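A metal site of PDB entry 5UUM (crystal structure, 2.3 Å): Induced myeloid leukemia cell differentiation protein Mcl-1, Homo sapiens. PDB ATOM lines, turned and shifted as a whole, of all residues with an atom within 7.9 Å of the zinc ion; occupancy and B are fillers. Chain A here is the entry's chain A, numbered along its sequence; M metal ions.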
ATOM      1  N   LYS A  39      13.725 -22.371 -19.482  1.00  0.00           N
ATOM      2  CA  LYS A  39      14.596 -21.450 -20.199  1.00  0.00           C
ATOM      3  C   LYS A  39      16.036 -21.941 -20.227  1.00  0.00           C
ATOM      4  O   LYS A  39      16.755 -21.694 -21.209  1.00  0.00           O
ATOM      5  CB  LYS A  39      14.504 -20.060 -19.564  1.00  0.00           C
ATOM      6  CG  LYS A  39      13.100 -19.454 -19.614  1.00  0.00           C
ATOM      7  CD  LYS A  39      12.990 -18.176 -18.807  1.00  0.00           C
ATOM      8  CE  LYS A  39      13.709 -17.021 -19.465  1.00  0.00           C
ATOM      9  NZ  LYS A  39      13.505 -15.749 -18.721  1.00  0.00           N
ATOM     10  N   ASP A 144      19.517 -19.522 -13.324  1.00  0.00           N
ATOM     11  CA  ASP A 144      19.124 -18.179 -13.744  1.00  0.00           C
ATOM     12  C   ASP A 144      20.329 -17.403 -14.268  1.00  0.00           C
ATOM     13  O   ASP A 144      20.229 -16.668 -15.258  1.00  0.00           O
ATOM     14  CB  ASP A 144      18.451 -17.429 -12.600  1.00  0.00           C
ATOM     15  CG  ASP A 144      17.105 -18.031 -12.217  1.00  0.00           C
ATOM     16  OD1 ASP A 144      16.302 -18.338 -13.119  1.00  0.00           O
ATOM     17  OD2 ASP A 144      16.859 -18.200 -10.994  1.00  0.00           O
ATOM     18  N   VAL A 147      21.229 -18.904 -17.716  1.00  0.00           N
ATOM     19  CA  VAL A 147      20.344 -18.389 -18.761  1.00  0.00           C
ATOM     20  C   VAL A 147      20.793 -16.994 -19.180  1.00  0.00           C
ATOM     21  O   VAL A 147      20.950 -16.707 -20.377  1.00  0.00           O
ATOM     22  CB  VAL A 147      18.882 -18.397 -18.272  1.00  0.00           C
ATOM     23  CG1 VAL A 147      17.993 -17.564 -19.192  1.00  0.00           C
ATOM     24  CG2 VAL A 147      18.367 -19.823 -18.195  1.00  0.00           C
ATOM     25  N   GLU A 148      20.981 -16.100 -18.204  1.00  0.00           N
ATOM     26  CA  GLU A 148      21.247 -14.697 -18.521  1.00  0.00           C
ATOM     27  C   GLU A 148      22.606 -14.520 -19.183  1.00  0.00           C
ATOM     28  O   GLU A 148      22.747 -13.750 -20.135  1.00  0.00           O
ATOM     29  CB  GLU A 148      21.147 -13.851 -17.249  1.00  0.00           C
ATOM     30  CG  GLU A 148      19.731 -13.748 -16.695  1.00  0.00           C
ATOM     31  CD  GLU A 148      18.758 -13.165 -17.703  1.00  0.00           C
ATOM     32  OE1 GLU A 148      19.143 -12.210 -18.414  1.00  0.00           O
ATOM     33  OE2 GLU A 148      17.615 -13.673 -17.798  1.00  0.00           O
ATOM     34  N   PHE A 149      23.628 -15.241 -18.704  1.00  0.00           N
ATOM     35  CA  PHE A 149      24.956 -15.108 -19.291  1.00  0.00           C
ATOM     36  C   PHE A 149      24.916 -15.323 -20.799  1.00  0.00           C
ATOM     37  O   PHE A 149      25.561 -14.589 -21.561  1.00  0.00           O
ATOM     38  CB  PHE A 149      25.912 -16.107 -18.636  1.00  0.00           C
ATOM     39  CG  PHE A 149      27.271 -16.139 -19.262  1.00  0.00           C
ATOM     40  CD1 PHE A 149      28.265 -15.275 -18.835  1.00  0.00           C
ATOM     41  CD2 PHE A 149      27.566 -17.037 -20.276  1.00  0.00           C
ATOM     42  CE1 PHE A 149      29.514 -15.296 -19.412  1.00  0.00           C
ATOM     43  CE2 PHE A 149      28.815 -17.069 -20.853  1.00  0.00           C
ATOM     44  CZ  PHE A 149      29.791 -16.203 -20.416  1.00  0.00           C
ATOM     45  N   PHE A 150      24.159 -16.325 -21.253  1.00  0.00           N
ATOM     46  CA  PHE A 150      24.069 -16.664 -22.664  1.00  0.00           C
ATOM     47  C   PHE A 150      22.886 -15.992 -23.362  1.00  0.00           C
ATOM     48  O   PHE A 150      22.587 -16.334 -24.509  1.00  0.00           O
ATOM     49  CB  PHE A 150      23.969 -18.180 -22.837  1.00  0.00           C
ATOM     50  CG  PHE A 150      25.224 -18.912 -22.475  1.00  0.00           C
ATOM     51  CD1 PHE A 150      26.369 -18.775 -23.247  1.00  0.00           C
ATOM     52  CD2 PHE A 150      25.268 -19.748 -21.362  1.00  0.00           C
ATOM     53  CE1 PHE A 150      27.528 -19.452 -22.924  1.00  0.00           C
ATOM     54  CE2 PHE A 150      26.426 -20.425 -21.039  1.00  0.00           C
ATOM     55  CZ  PHE A 150      27.559 -20.277 -21.815  1.00  0.00           C
ATOM     56  N   HIS A 151      22.202 -15.062 -22.704  1.00  0.00           N
ATOM     57  CA  HIS A 151      21.051 -14.387 -23.284  1.00  0.00           C
ATOM     58  C   HIS A 151      21.497 -13.093 -23.940  1.00  0.00           C
ATOM     59  O   HIS A 151      22.010 -12.185 -23.270  1.00  0.00           O
ATOM     60  CB  HIS A 151      19.992 -14.106 -22.219  1.00  0.00           C
ATOM     61  CG  HIS A 151      18.745 -13.472 -22.757  1.00  0.00           C
ATOM     62  ND1 HIS A 151      18.070 -12.473 -22.093  1.00  0.00           N
ATOM     63  CD2 HIS A 151      18.065 -13.678 -23.911  1.00  0.00           C
ATOM     64  CE1 HIS A 151      17.019 -12.101 -22.794  1.00  0.00           C
ATOM     65  NE2 HIS A 151      16.999 -12.822 -23.910  1.00  0.00           N
ATOM     66  N   VAL A 152      21.286 -12.987 -25.252  1.00  0.00           N
ATOM     67  CA  VAL A 152      21.606 -11.778 -25.998  1.00  0.00           C
ATOM     68  C   VAL A 152      20.487 -10.779 -25.786  1.00  0.00           C
ATOM     69  O   VAL A 152      19.328 -11.055 -26.114  1.00  0.00           O
ATOM     70  CB  VAL A 152      21.812 -12.080 -27.482  1.00  0.00           C
ATOM     71  CG1 VAL A 152      22.350 -10.855 -28.211  1.00  0.00           C
ATOM     72  CG2 VAL A 152      22.749 -13.266 -27.660  1.00  0.00           C
ATOM     73  N   GLU A 153      20.825  -9.604 -25.250  1.00  0.00           N
ATOM     74  CA  GLU A 153      19.815  -8.652 -24.812  1.00  0.00           C
ATOM     75  C   GLU A 153      19.430  -7.640 -25.886  1.00  0.00           C
ATOM     76  O   GLU A 153      18.318  -7.100 -25.834  1.00  0.00           O
ATOM     77  CB  GLU A 153      20.298  -7.916 -23.564  1.00  0.00           C
ATOM     78  CG  GLU A 153      20.441  -8.814 -22.345  1.00  0.00           C
ATOM     79  CD  GLU A 153      19.105  -9.291 -21.819  1.00  0.00           C
ATOM     80  OE1 GLU A 153      18.066  -8.873 -22.379  1.00  0.00           O
ATOM     81  OE2 GLU A 153      19.089 -10.068 -20.845  1.00  0.00           O
HETATM   82 ZN    ZN M   1      18.228 -11.519 -20.290  1.00  0.00          ZN
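The zinc ion is bound by the side-chain carboxylate of Glu 153 (1.8 Å), a ring nitrogen (ND1) of His 151 (2.0 Å) and the side-chain carboxylate of Glu 148 (2.2 Å).
The zinc ion has three donor atoms within binding distance.
Within 4 Å of the zinc ion: Glu 148, His 151 and Glu 153.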
